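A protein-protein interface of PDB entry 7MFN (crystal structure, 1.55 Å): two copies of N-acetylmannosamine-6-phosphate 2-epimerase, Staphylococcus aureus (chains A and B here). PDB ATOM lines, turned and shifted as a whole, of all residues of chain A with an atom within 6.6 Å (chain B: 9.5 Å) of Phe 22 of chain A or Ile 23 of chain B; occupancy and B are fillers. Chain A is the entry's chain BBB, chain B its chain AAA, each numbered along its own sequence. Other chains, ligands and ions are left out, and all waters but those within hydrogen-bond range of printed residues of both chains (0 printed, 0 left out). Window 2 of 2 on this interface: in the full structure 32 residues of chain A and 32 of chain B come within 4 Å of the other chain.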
ATOM      1  N   LEU A  18      -4.301 -15.394  28.186  1.00  0.00           N
ATOM      2  CA  LEU A  18      -3.487 -16.186  27.233  1.00  0.00           C
ATOM      3  C   LEU A  18      -1.971 -15.963  27.419  1.00  0.00           C
ATOM      4  O   LEU A  18      -1.219 -16.384  26.542  1.00  0.00           O
ATOM      5  CB  LEU A  18      -3.910 -15.870  25.811  1.00  0.00           C
ATOM      6  CG  LEU A  18      -5.379 -16.093  25.478  1.00  0.00           C
ATOM      7  CD1 LEU A  18      -5.576 -15.982  23.973  1.00  0.00           C
ATOM      8  CD2 LEU A  18      -5.846 -17.449  26.005  1.00  0.00           C
ATOM      9  N   SER A  20       1.546 -16.523  27.592  1.00  0.00           N
ATOM     10  CA  SER A  20       2.230 -17.786  27.213  1.00  0.00           C
ATOM     11  C   SER A  20       2.971 -17.546  25.908  1.00  0.00           C
ATOM     12  O   SER A  20       2.271 -17.188  24.907  1.00  0.00           O
ATOM     13  CB  SER A  20       1.272 -18.913  27.012  1.00  0.00           C
ATOM     14  OG  SER A  20       1.929 -19.979  26.390  1.00  0.00           O
ATOM     15  N   SER A  21       4.287 -17.791  25.856  1.00  0.00           N
ATOM     16  CA  SER A  21       5.035 -17.794  24.576  1.00  0.00           C
ATOM     17  C   SER A  21       4.463 -18.824  23.605  1.00  0.00           C
ATOM     18  O   SER A  21       4.298 -18.569  22.408  1.00  0.00           O
ATOM     19  CB  SER A  21       6.517 -17.983  24.785  1.00  0.00           C
ATOM     20  OG  SER A  21       6.999 -16.981  25.662  1.00  0.00           O
ATOM     21  N   PHE A  22       4.132 -20.022  24.103  1.00  0.00           N
ATOM     22  CA  PHE A  22       3.542 -21.075  23.267  1.00  0.00           C
ATOM     23  C   PHE A  22       2.208 -20.585  22.705  1.00  0.00           C
ATOM     24  O   PHE A  22       1.973 -20.693  21.506  1.00  0.00           O
ATOM     25  CB  PHE A  22       3.349 -22.358  24.075  1.00  0.00           C
ATOM     26  CG  PHE A  22       2.860 -23.507  23.251  1.00  0.00           C
ATOM     27  CD1 PHE A  22       3.757 -24.307  22.561  1.00  0.00           C
ATOM     28  CD2 PHE A  22       1.534 -23.820  23.159  1.00  0.00           C
ATOM     29  CE1 PHE A  22       3.332 -25.367  21.785  1.00  0.00           C
ATOM     30  CE2 PHE A  22       1.105 -24.866  22.344  1.00  0.00           C
ATOM     31  CZ  PHE A  22       2.000 -25.656  21.683  1.00  0.00           C
ATOM     32  N   ILE A  23       1.290 -20.088  23.521  1.00  0.00           N
ATOM     33  CA  ILE A  23      -0.003 -19.657  22.949  1.00  0.00           C
ATOM     34  C   ILE A  23       0.211 -18.538  21.929  1.00  0.00           C
ATOM     35  O   ILE A  23      -0.435 -18.553  20.867  1.00  0.00           O
ATOM     36  CB  ILE A  23      -1.034 -19.305  24.005  1.00  0.00           C
ATOM     37  CG1 ILE A  23      -1.245 -20.492  24.974  1.00  0.00           C
ATOM     38  CG2 ILE A  23      -2.325 -18.887  23.362  1.00  0.00           C
ATOM     39  CD1 ILE A  23      -2.223 -20.135  26.074  1.00  0.00           C
ATOM     40  N   MET A  24       1.045 -17.562  22.255  1.00  0.00           N
ATOM     41  CA  MET A  24       1.212 -16.484  21.229  1.00  0.00           C
ATOM     42  C   MET A  24       1.833 -17.041  19.953  1.00  0.00           C
ATOM     43  O   MET A  24       1.495 -16.504  18.854  1.00  0.00           O
ATOM     44  CB  MET A  24       2.047 -15.335  21.789  1.00  0.00           C
ATOM     45  CG  MET A  24       1.318 -14.586  22.915  1.00  0.00           C
ATOM     46  SD  MET A  24      -0.250 -13.869  22.489  1.00  0.00           S
ATOM     47  CE  MET A  24      -1.375 -15.083  23.205  1.00  0.00           C
ATOM     48  N   SER A  25       2.705 -18.054  20.010  1.00  0.00           N
ATOM     49  CA  SER A  25       3.247 -18.655  18.788  1.00  0.00           C
ATOM     50  C   SER A  25       2.113 -19.265  17.953  1.00  0.00           C
ATOM     51  O   SER A  25       2.165 -19.253  16.722  1.00  0.00           O
ATOM     52  CB  SER A  25       4.370 -19.642  19.097  1.00  0.00           C
ATOM     53  OG  SER A  25       3.865 -20.889  19.625  1.00  0.00           O
ATOM     54  N   LYS A  26       1.078 -19.826  18.590  1.00  0.00           N
ATOM     55  CA  LYS A  26      -0.067 -20.434  17.880  1.00  0.00           C
ATOM     56  C   LYS A  26      -1.043 -19.392  17.370  1.00  0.00           C
ATOM     57  O   LYS A  26      -1.579 -19.553  16.273  1.00  0.00           O
ATOM     58  CB  LYS A  26      -0.773 -21.480  18.758  1.00  0.00           C
ATOM     59  CG  LYS A  26       0.140 -22.614  19.154  1.00  0.00           C
ATOM     60  CD  LYS A  26       0.770 -23.307  17.971  1.00  0.00           C
ATOM     61  CE  LYS A  26       1.626 -24.457  18.431  1.00  0.00           C
ATOM     62  NZ  LYS A  26       2.083 -25.219  17.259  1.00  0.00           N
ATOM     63  N   MET A  27      -1.172 -18.269  18.077  1.00  0.00           N
ATOM     64  CA  MET A  27      -1.885 -17.090  17.537  1.00  0.00           C
ATOM     65  C   MET A  27      -1.189 -16.631  16.249  1.00  0.00           C
ATOM     66  O   MET A  27      -1.894 -16.321  15.270  1.00  0.00           O
ATOM     67  CB  MET A  27      -1.924 -15.934  18.540  1.00  0.00           C
ATOM     68  CG  MET A  27      -2.909 -16.156  19.706  1.00  0.00           C
ATOM     69  SD  MET A  27      -4.590 -16.078  19.106  1.00  0.00           S
ATOM     70  CE  MET A  27      -5.521 -16.209  20.646  1.00  0.00           C
ATOM     71  N   GLU A  45      11.064 -13.852  24.742  1.00  0.00           N
ATOM     72  CA  GLU A  45      10.598 -15.268  24.807  1.00  0.00           C
ATOM     73  C   GLU A  45       9.435 -15.472  23.827  1.00  0.00           C
ATOM     74  O   GLU A  45       9.429 -16.460  23.068  1.00  0.00           O
ATOM     75  CB  GLU A  45      10.160 -15.616  26.219  1.00  0.00           C
ATOM     76  CG  GLU A  45      11.282 -15.500  27.257  1.00  0.00           C
ATOM     77  CD  GLU A  45      11.807 -14.115  27.657  1.00  0.00           C
ATOM     78  OE1 GLU A  45      11.044 -13.049  27.559  1.00  0.00           O
ATOM     79  OE2 GLU A  45      13.017 -14.083  28.060  1.00  0.00           O
ATOM     80  N   ASP A  46       8.477 -14.538  23.800  1.00  0.00           N
ATOM     81  CA  ASP A  46       7.376 -14.696  22.818  1.00  0.00           C
ATOM     82  C   ASP A  46       7.903 -14.615  21.386  1.00  0.00           C
ATOM     83  O   ASP A  46       7.504 -15.360  20.489  1.00  0.00           O
ATOM     84  CB  ASP A  46       6.236 -13.698  23.039  1.00  0.00           C
ATOM     85  CG  ASP A  46       5.340 -13.939  24.235  1.00  0.00           C
ATOM     86  OD1 ASP A  46       5.778 -14.658  25.141  1.00  0.00           O
ATOM     87  OD2 ASP A  46       4.290 -13.272  24.335  1.00  0.00           O
ATOM     88  N   ALA A  49       9.745 -17.742  20.186  1.00  0.00           N
ATOM     89  CA  ALA A  49       8.778 -18.841  19.955  1.00  0.00           C
ATOM     90  C   ALA A  49       8.080 -18.625  18.621  1.00  0.00           C
ATOM     91  O   ALA A  49       7.872 -19.571  17.840  1.00  0.00           O
ATOM     92  CB  ALA A  49       7.779 -18.953  21.057  1.00  0.00           C
ATOM     93  N   THR A  53       8.106 -20.660  14.649  1.00  0.00           N
ATOM     94  CA  THR A  53       6.788 -21.203  14.237  1.00  0.00           C
ATOM     95  C   THR A  53       6.416 -20.684  12.840  1.00  0.00           C
ATOM     96  O   THR A  53       5.826 -21.433  12.052  1.00  0.00           O
ATOM     97  CB  THR A  53       5.794 -20.833  15.333  1.00  0.00           C
ATOM     98  OG1 THR A  53       6.166 -21.311  16.620  1.00  0.00           O
ATOM     99  CG2 THR A  53       4.385 -21.316  15.056  1.00  0.00           C
ATOM    100  N   CYS B  10     -15.477 -22.768  22.634  1.00  0.00           N
ATOM    101  CA  CYS B  10     -13.988 -22.823  22.792  1.00  0.00           C
ATOM    102  C   CYS B  10     -13.543 -24.196  22.228  1.00  0.00           C
ATOM    103  O   CYS B  10     -13.304 -25.119  23.011  1.00  0.00           O
ATOM    104  CB  CYS B  10     -13.599 -22.658  24.246  1.00  0.00           C
ATOM    105  SG  CYS B  10     -14.051 -21.046  24.908  1.00  0.00           S
ATOM    106  N   GLN B  11     -13.450 -24.299  20.919  1.00  0.00           N
ATOM    107  CA  GLN B  11     -13.080 -25.525  20.214  1.00  0.00           C
ATOM    108  C   GLN B  11     -11.862 -25.270  19.327  1.00  0.00           C
ATOM    109  O   GLN B  11     -11.729 -24.228  18.703  1.00  0.00           O
ATOM    110  CB  GLN B  11     -14.254 -26.047  19.398  1.00  0.00           C
ATOM    111  CG  GLN B  11     -15.476 -26.403  20.239  1.00  0.00           C
ATOM    112  CD  GLN B  11     -16.552 -27.014  19.391  1.00  0.00           C
ATOM    113  OE1 GLN B  11     -16.322 -27.958  18.636  1.00  0.00           O
ATOM    114  NE2 GLN B  11     -17.741 -26.435  19.457  1.00  0.00           N
ATOM    115  N   ALA B  12     -11.075 -26.318  19.171  1.00  0.00           N
ATOM    116  CA  ALA B  12      -9.902 -26.330  18.270  1.00  0.00           C
ATOM    117  C   ALA B  12      -9.595 -27.813  18.011  1.00  0.00           C
ATOM    118  O   ALA B  12      -9.084 -28.473  18.884  1.00  0.00           O
ATOM    119  CB  ALA B  12      -8.752 -25.591  18.892  1.00  0.00           C
ATOM    120  N   GLU B  16      -5.844 -27.750  14.087  1.00  0.00           N
ATOM    121  CA  GLU B  16      -6.117 -26.283  14.166  1.00  0.00           C
ATOM    122  C   GLU B  16      -5.026 -25.696  15.041  1.00  0.00           C
ATOM    123  O   GLU B  16      -4.543 -26.297  15.995  1.00  0.00           O
ATOM    124  CB  GLU B  16      -7.483 -25.967  14.778  1.00  0.00           C
ATOM    125  CG  GLU B  16      -8.715 -26.283  13.928  1.00  0.00           C
ATOM    126  CD  GLU B  16     -10.019 -25.643  14.481  1.00  0.00           C
ATOM    127  OE1 GLU B  16     -10.113 -24.352  14.525  1.00  0.00           O
ATOM    128  OE2 GLU B  16     -10.966 -26.390  14.920  1.00  0.00           O
ATOM    129  N   PRO B  17      -4.659 -24.399  14.844  1.00  0.00           N
ATOM    130  CA  PRO B  17      -3.544 -23.840  15.604  1.00  0.00           C
ATOM    131  C   PRO B  17      -3.617 -23.918  17.120  1.00  0.00           C
ATOM    132  O   PRO B  17      -2.601 -24.171  17.723  1.00  0.00           O
ATOM    133  CB  PRO B  17      -3.622 -22.345  15.232  1.00  0.00           C
ATOM    134  CG  PRO B  17      -4.168 -22.362  13.849  1.00  0.00           C
ATOM    135  CD  PRO B  17      -5.197 -23.499  13.836  1.00  0.00           C
ATOM    136  N   LEU B  18      -4.816 -23.688  17.703  1.00  0.00           N
ATOM    137  CA  LEU B  18      -4.960 -23.628  19.151  1.00  0.00           C
ATOM    138  C   LEU B  18      -5.372 -24.995  19.740  1.00  0.00           C
ATOM    139  O   LEU B  18      -5.634 -25.023  20.931  1.00  0.00           O
ATOM    140  CB  LEU B  18      -5.999 -22.565  19.514  1.00  0.00           C
ATOM    141  CG  LEU B  18      -5.683 -21.132  19.080  1.00  0.00           C
ATOM    142  CD1 LEU B  18      -6.802 -20.215  19.554  1.00  0.00           C
ATOM    143  CD2 LEU B  18      -4.346 -20.668  19.646  1.00  0.00           C
ATOM    144  N   HIS B  19      -5.269 -26.077  18.967  1.00  0.00           N
ATOM    145  CA  HIS B  19      -5.621 -27.425  19.467  1.00  0.00           C
ATOM    146  C   HIS B  19      -4.851 -27.707  20.745  1.00  0.00           C
ATOM    147  O   HIS B  19      -3.594 -27.760  20.692  1.00  0.00           O
ATOM    148  CB  HIS B  19      -5.428 -28.477  18.377  1.00  0.00           C
ATOM    149  CG  HIS B  19      -5.653 -29.874  18.838  1.00  0.00           C
ATOM    150  ND1 HIS B  19      -6.913 -30.348  19.158  1.00  0.00           N
ATOM    151  CD2 HIS B  19      -4.795 -30.881  19.032  1.00  0.00           C
ATOM    152  CE1 HIS B  19      -6.802 -31.647  19.491  1.00  0.00           C
ATOM    153  NE2 HIS B  19      -5.523 -31.988  19.424  1.00  0.00           N
ATOM    154  N   SER B  20      -5.562 -27.914  21.858  1.00  0.00           N
ATOM    155  CA  SER B  20      -5.004 -28.061  23.220  1.00  0.00           C
ATOM    156  C   SER B  20      -6.126 -27.924  24.230  1.00  0.00           C
ATOM    157  O   SER B  20      -6.732 -26.839  24.255  1.00  0.00           O
ATOM    158  CB  SER B  20      -3.916 -27.018  23.587  1.00  0.00           C
ATOM    159  OG  SER B  20      -3.637 -27.125  24.957  1.00  0.00           O
ATOM    160  N   SER B  21      -6.322 -28.899  25.095  1.00  0.00           N
ATOM    161  CA  SER B  21      -7.251 -28.801  26.217  1.00  0.00           C
ATOM    162  C   SER B  21      -6.884 -27.591  27.098  1.00  0.00           C
ATOM    163  O   SER B  21      -7.752 -26.836  27.537  1.00  0.00           O
ATOM    164  CB  SER B  21      -7.306 -30.068  27.038  1.00  0.00           C
ATOM    165  OG  SER B  21      -7.755 -31.136  26.230  1.00  0.00           O
ATOM    166  N   PHE B  22      -5.570 -27.432  27.308  1.00  0.00           N
ATOM    167  CA  PHE B  22      -4.965 -26.328  28.099  1.00  0.00           C
ATOM    168  C   PHE B  22      -5.408 -25.002  27.527  1.00  0.00           C
ATOM    169  O   PHE B  22      -6.027 -24.195  28.265  1.00  0.00           O
ATOM    170  CB  PHE B  22      -3.429 -26.313  28.031  1.00  0.00           C
ATOM    171  CG  PHE B  22      -2.805 -25.158  28.779  1.00  0.00           C
ATOM    172  CD1 PHE B  22      -2.814 -25.118  30.167  1.00  0.00           C
ATOM    173  CD2 PHE B  22      -2.237 -24.107  28.106  1.00  0.00           C
ATOM    174  CE1 PHE B  22      -2.236 -24.058  30.853  1.00  0.00           C
ATOM    175  CE2 PHE B  22      -1.666 -23.048  28.794  1.00  0.00           C
ATOM    176  CZ  PHE B  22      -1.652 -23.036  30.158  1.00  0.00           C
ATOM    177  N   ILE B  23      -5.089 -24.807  26.260  1.00  0.00           N
ATOM    178  CA  ILE B  23      -5.358 -23.547  25.535  1.00  0.00           C
ATOM    179  C   ILE B  23      -6.881 -23.282  25.566  1.00  0.00           C
ATOM    180  O   ILE B  23      -7.277 -22.168  25.837  1.00  0.00           O
ATOM    181  CB  ILE B  23      -4.771 -23.456  24.135  1.00  0.00           C
ATOM    182  CG1 ILE B  23      -3.250 -23.646  24.211  1.00  0.00           C
ATOM    183  CG2 ILE B  23      -5.155 -22.166  23.505  1.00  0.00           C
ATOM    184  CD1 ILE B  23      -2.628 -23.654  22.882  1.00  0.00           C
ATOM    185  N   MET B  24      -7.717 -24.292  25.292  1.00  0.00           N
ATOM    186  CA  MET B  24      -9.188 -24.027  25.336  1.00  0.00           C
ATOM    187  C   MET B  24      -9.580 -23.592  26.740  1.00  0.00           C
ATOM    188  O   MET B  24     -10.543 -22.780  26.835  1.00  0.00           O
ATOM    189  CB  MET B  24      -9.975 -25.255  24.872  1.00  0.00           C
ATOM    190  CG  MET B  24      -9.826 -25.503  23.372  1.00  0.00           C
ATOM    191  SD  MET B  24     -10.236 -24.178  22.251  1.00  0.00           S
ATOM    192  CE  MET B  24      -8.623 -23.424  21.968  1.00  0.00           C
ATOM    193  N   SER B  25      -8.977 -24.114  27.787  1.00  0.00           N
ATOM    194  CA  SER B  25      -9.294 -23.670  29.164  1.00  0.00           C
ATOM    195  C   SER B  25      -8.981 -22.173  29.331  1.00  0.00           C
ATOM    196  O   SER B  25      -9.706 -21.501  30.061  1.00  0.00           O
ATOM    197  CB  SER B  25      -8.700 -24.537  30.274  1.00  0.00           C
ATOM    198  OG  SER B  25      -7.293 -24.260  30.462  1.00  0.00           O
ATOM    199  N   LYS B  26      -7.845 -21.694  28.807  1.00  0.00           N
ATOM    200  CA  LYS B  26      -7.500 -20.270  28.977  1.00  0.00           C
ATOM    201  C   LYS B  26      -8.431 -19.433  28.082  1.00  0.00           C
ATOM    202  O   LYS B  26      -8.783 -18.319  28.492  1.00  0.00           O
ATOM    203  CB  LYS B  26      -5.992 -20.089  28.759  1.00  0.00           C
ATOM    204  CG  LYS B  26      -5.124 -20.652  29.875  1.00  0.00           C
ATOM    205  CD  LYS B  26      -5.482 -20.036  31.212  1.00  0.00           C
ATOM    206  CE  LYS B  26      -4.653 -20.421  32.426  1.00  0.00           C
ATOM    207  NZ  LYS B  26      -5.419 -20.064  33.638  1.00  0.00           N
ATOM    208  N   MET B  27      -8.836 -19.926  26.918  1.00  0.00           N
ATOM    209  CA  MET B  27      -9.821 -19.225  26.055  1.00  0.00           C
ATOM    210  C   MET B  27     -11.153 -19.090  26.827  1.00  0.00           C
ATOM    211  O   MET B  27     -11.742 -17.989  26.843  1.00  0.00           O
ATOM    212  CB  MET B  27     -10.081 -19.949  24.733  1.00  0.00           C
ATOM    213  CG  MET B  27      -8.836 -20.215  23.869  1.00  0.00           C
ATOM    214  SD  MET B  27      -8.074 -18.703  23.226  1.00  0.00           S
ATOM    215  CE  MET B  27      -9.212 -18.217  21.926  1.00  0.00           C
ATOM    216  N   ALA B  28     -11.608 -20.162  27.488  1.00  0.00           N
ATOM    217  CA  ALA B  28     -12.858 -20.124  28.287  1.00  0.00           C
ATOM    218  C   ALA B  28     -12.726 -19.118  29.439  1.00  0.00           C
ATOM    219  O   ALA B  28     -13.722 -18.419  29.751  1.00  0.00           O
ATOM    220  CB  ALA B  28     -13.201 -21.502  28.809  1.00  0.00           C
ATOM    221  N   LEU B  29     -11.562 -19.034  30.072  1.00  0.00           N
ATOM    222  CA  LEU B  29     -11.295 -18.023  31.103  1.00  0.00           C
ATOM    223  C   LEU B  29     -11.496 -16.635  30.506  1.00  0.00           C
ATOM    224  O   LEU B  29     -12.109 -15.766  31.126  1.00  0.00           O
ATOM    225  CB  LEU B  29      -9.887 -18.215  31.671  1.00  0.00           C
ATOM    226  CG  LEU B  29      -9.549 -17.209  32.758  1.00  0.00           C
ATOM    227  CD1 LEU B  29     -10.481 -17.271  33.958  1.00  0.00           C
ATOM    228  CD2 LEU B  29      -8.099 -17.460  33.210  1.00  0.00           C
ATOM    229  N   ALA B  30     -10.921 -16.384  29.308  1.00  0.00           N
ATOM    230  CA  ALA B  30     -11.052 -15.083  28.661  1.00  0.00           C
ATOM    231  C   ALA B  30     -12.524 -14.785  28.411  1.00  0.00           C
ATOM    232  O   ALA B  30     -12.964 -13.672  28.659  1.00  0.00           O
ATOM    233  CB  ALA B  30     -10.236 -15.119  27.366  1.00  0.00           C
ATOM    234  N   ALA B  31     -13.284 -15.771  27.954  1.00  0.00           N
ATOM    235  CA  ALA B  31     -14.736 -15.599  27.645  1.00  0.00           C
ATOM    236  C   ALA B  31     -15.454 -15.250  28.970  1.00  0.00           C
ATOM    237  O   ALA B  31     -16.294 -14.310  28.988  1.00  0.00           O
ATOM    238  CB  ALA B  31     -15.272 -16.852  27.019  1.00  0.00           C
ATOM    239  N   GLU B  45     -11.784 -34.311  27.572  1.00  0.00           N
ATOM    240  CA  GLU B  45     -10.514 -33.745  28.074  1.00  0.00           C
ATOM    241  C   GLU B  45     -10.577 -32.207  28.030  1.00  0.00           C
ATOM    242  O   GLU B  45     -10.189 -31.572  29.024  1.00  0.00           O
ATOM    243  CB  GLU B  45      -9.361 -34.310  27.265  1.00  0.00           C
ATOM    244  CG  GLU B  45      -9.074 -35.772  27.586  1.00  0.00           C
ATOM    245  CD  GLU B  45     -10.039 -36.767  26.937  1.00  0.00           C
ATOM    246  OE1 GLU B  45     -10.715 -36.425  25.937  1.00  0.00           O
ATOM    247  OE2 GLU B  45     -10.063 -37.894  27.440  1.00  0.00           O
ATOM    248  N   ASP B  46     -11.111 -31.630  26.964  1.00  0.00           N
ATOM    249  CA  ASP B  46     -11.201 -30.147  26.921  1.00  0.00           C
ATOM    250  C   ASP B  46     -12.201 -29.691  27.976  1.00  0.00           C
ATOM    251  O   ASP B  46     -11.972 -28.662  28.656  1.00  0.00           O
ATOM    252  CB  ASP B  46     -11.632 -29.584  25.571  1.00  0.00           C
ATOM    253  CG  ASP B  46     -10.575 -29.628  24.476  1.00  0.00           C
ATOM    254  OD1 ASP B  46      -9.640 -30.482  24.588  1.00  0.00           O
ATOM    255  OD2 ASP B  46     -10.746 -28.919  23.460  1.00  0.00           O
ATOM    256  N   ALA B  49     -10.631 -29.740  31.435  1.00  0.00           N
ATOM    257  CA  ALA B  49      -9.631 -28.651  31.577  1.00  0.00           C
ATOM    258  C   ALA B  49     -10.385 -27.328  31.824  1.00  0.00           C
ATOM    259  O   ALA B  49     -10.018 -26.551  32.696  1.00  0.00           O
ATOM    260  CB  ALA B  49      -8.740 -28.575  30.365  1.00  0.00           C
ATOM    261  N   ILE B  50     -11.400 -27.044  31.004  1.00  0.00           N
ATOM    262  CA  ILE B  50     -12.227 -25.831  31.144  1.00  0.00           C
ATOM    263  C   ILE B  50     -12.847 -25.779  32.525  1.00  0.00           C
ATOM    264  O   ILE B  50     -12.887 -24.711  33.131  1.00  0.00           O
ATOM    265  CB  ILE B  50     -13.271 -25.786  30.025  1.00  0.00           C
ATOM    266  CG1 ILE B  50     -12.607 -25.501  28.680  1.00  0.00           C
ATOM    267  CG2 ILE B  50     -14.392 -24.796  30.335  1.00  0.00           C
ATOM    268  CD1 ILE B  50     -13.442 -25.865  27.495  1.00  0.00           C
ATOM    269  N   THR B  53     -10.686 -24.020  35.064  1.00  0.00           N
ATOM    270  CA  THR B  53     -10.493 -22.546  35.006  1.00  0.00           C
ATOM    271  C   THR B  53     -11.792 -21.815  35.313  1.00  0.00           C
ATOM    272  O   THR B  53     -11.685 -20.731  35.883  1.00  0.00           O
ATOM    273  CB  THR B  53      -9.912 -21.980  33.700  1.00  0.00           C
ATOM    274  OG1 THR B  53     -10.769 -22.306  32.595  1.00  0.00           O
ATOM    275  CG2 THR B  53      -8.502 -22.494  33.504  1.00  0.00           C
ATOM    276  N   THR B 207     -12.898 -17.239  19.142  1.00  0.00           N
ATOM    277  CA  THR B 207     -11.863 -18.219  19.526  1.00  0.00           C
ATOM    278  C   THR B 207     -11.142 -18.868  18.336  1.00  0.00           C
ATOM    279  O   THR B 207     -10.343 -19.752  18.624  1.00  0.00           O
ATOM    280  CB  THR B 207     -12.473 -19.316  20.413  1.00  0.00           C
ATOM    281  OG1 THR B 207     -13.469 -20.033  19.695  1.00  0.00           O
ATOM    282  CG2 THR B 207     -13.084 -18.737  21.672  1.00  0.00           C
ATOM    283  N   PRO B 209      -8.727 -17.318  15.767  1.00  0.00           N
ATOM    284  CA  PRO B 209      -7.993 -16.194  15.168  1.00  0.00           C
ATOM    285  C   PRO B 209      -7.730 -16.368  13.666  1.00  0.00           C
ATOM    286  O   PRO B 209      -7.685 -15.350  12.960  1.00  0.00           O
ATOM    287  CB  PRO B 209      -6.701 -16.114  15.986  1.00  0.00           C
ATOM    288  CG  PRO B 209      -6.574 -17.466  16.626  1.00  0.00           C
ATOM    289  CD  PRO B 209      -8.016 -17.848  16.939  1.00  0.00           C
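Leu 18 of chain A touches Lys 26 of chain B, and with the chains exchanged Lys 26 of chain A touches Leu 18 of chain B. Leu 18 of chain A touches Met 27 of chain B, but with the chains exchanged Met 27 of chain A does not touch Leu 18 of chain B (4.3 Å). Phe 22 of chain A touches Ile 23 of chain B, but with the chains exchanged Ile 23 of chain A does not touch Phe 22 of chain B (4.02 Å). Ile 23 of chain A touches its own counterpart, Ile 23 of chain B. 13 positions are printed for both chains. Of the 7 pairs that touch across the chains among the printed residues, 3 have their exchanged pair printed and touching as well.
Among the printed residues, pairs that only touch across the chains: Leu 18 of chain A with Lys 26 of chain B, Leu 18 of chain A with Met 27 of chain B, Phe 22 of chain A with Ile 23 of chain B, Ile 23 of chain A with Ile 23 of chain B, Lys 26 of chain A with Pro 17 of chain B, Lys 26 of chain A with Leu 18 of chain B and Met 27 of chain A with Pro 209 of chain B.
No residue of chain B comes within 4 Å of Ser 21 of chain A. Of chain B, only Ile 23 (3.96 Å) comes within 4 Å of Phe 22 of chain A. Of chain B, only Ile 23 comes within 4 Å of Ile 23 of chain A. Met 24 of chain A touches none of the printed residues of chain B. No residue of chain B comes within 4 Å of Ser 25 of chain A. Of the printed residues of chain B, Lys 26 of chain A touches Pro 17 (3.4 Å) and Leu 18 (3.8 Å). Glu 45 of chain A touches none of the printed residues of chain B. Of chain A, only Phe 22 (3.96 Å) and Ile 23 (3.8 Å) come within 4 Å of Ile 23 of chain B. Printed residues of chain A within 4 Å of Lys 26 of chain B: Leu 18 (3.8 Å). Of the printed residues of chain A, Pro 209 of chain B touches Met 27 (3.5 Å). The nearest printed residue of chain A that does not touch Lys 26 of chain B is Ile 23 of chain A (4.6 Å).
Hydrophobic or aromatic side chains of chain B within 4 Å of the printed part of chain A: Pro 17, Leu 18, Ile 23, Met 27 and Pro 209. Hydrophobic or aromatic side chains of chain A that line the printed part of chain B: Leu 18, Phe 22, Ile 23 and Met 27. Among the printed residues, no Asp or Glu carboxylate lies within 4 Å of a Lys or Arg side-chain nitrogen of the other chain.
The side-chain hydroxyl (OG) of Ser 20 of chain A lies within hydrogen-bond range of the backbone NH (N) of Phe 22 of chain A (3.2 Å). The backbone NH of Ile 23 of chain A sits at hydrogen-bond distance from the side-chain hydroxyl of Ser 20 of chain A, at 2.9 Å. The backbone carbonyl oxygen of Phe 22 of chain A lies within hydrogen-bond range of the side-chain hydroxyl of Ser 25 of chain A (2.7 Å). The backbone NH (N) of Ile 23 of chain B is in hydrogen-bond range of the side-chain hydroxyl (OG) of Ser 20 of chain B (3.0 Å).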
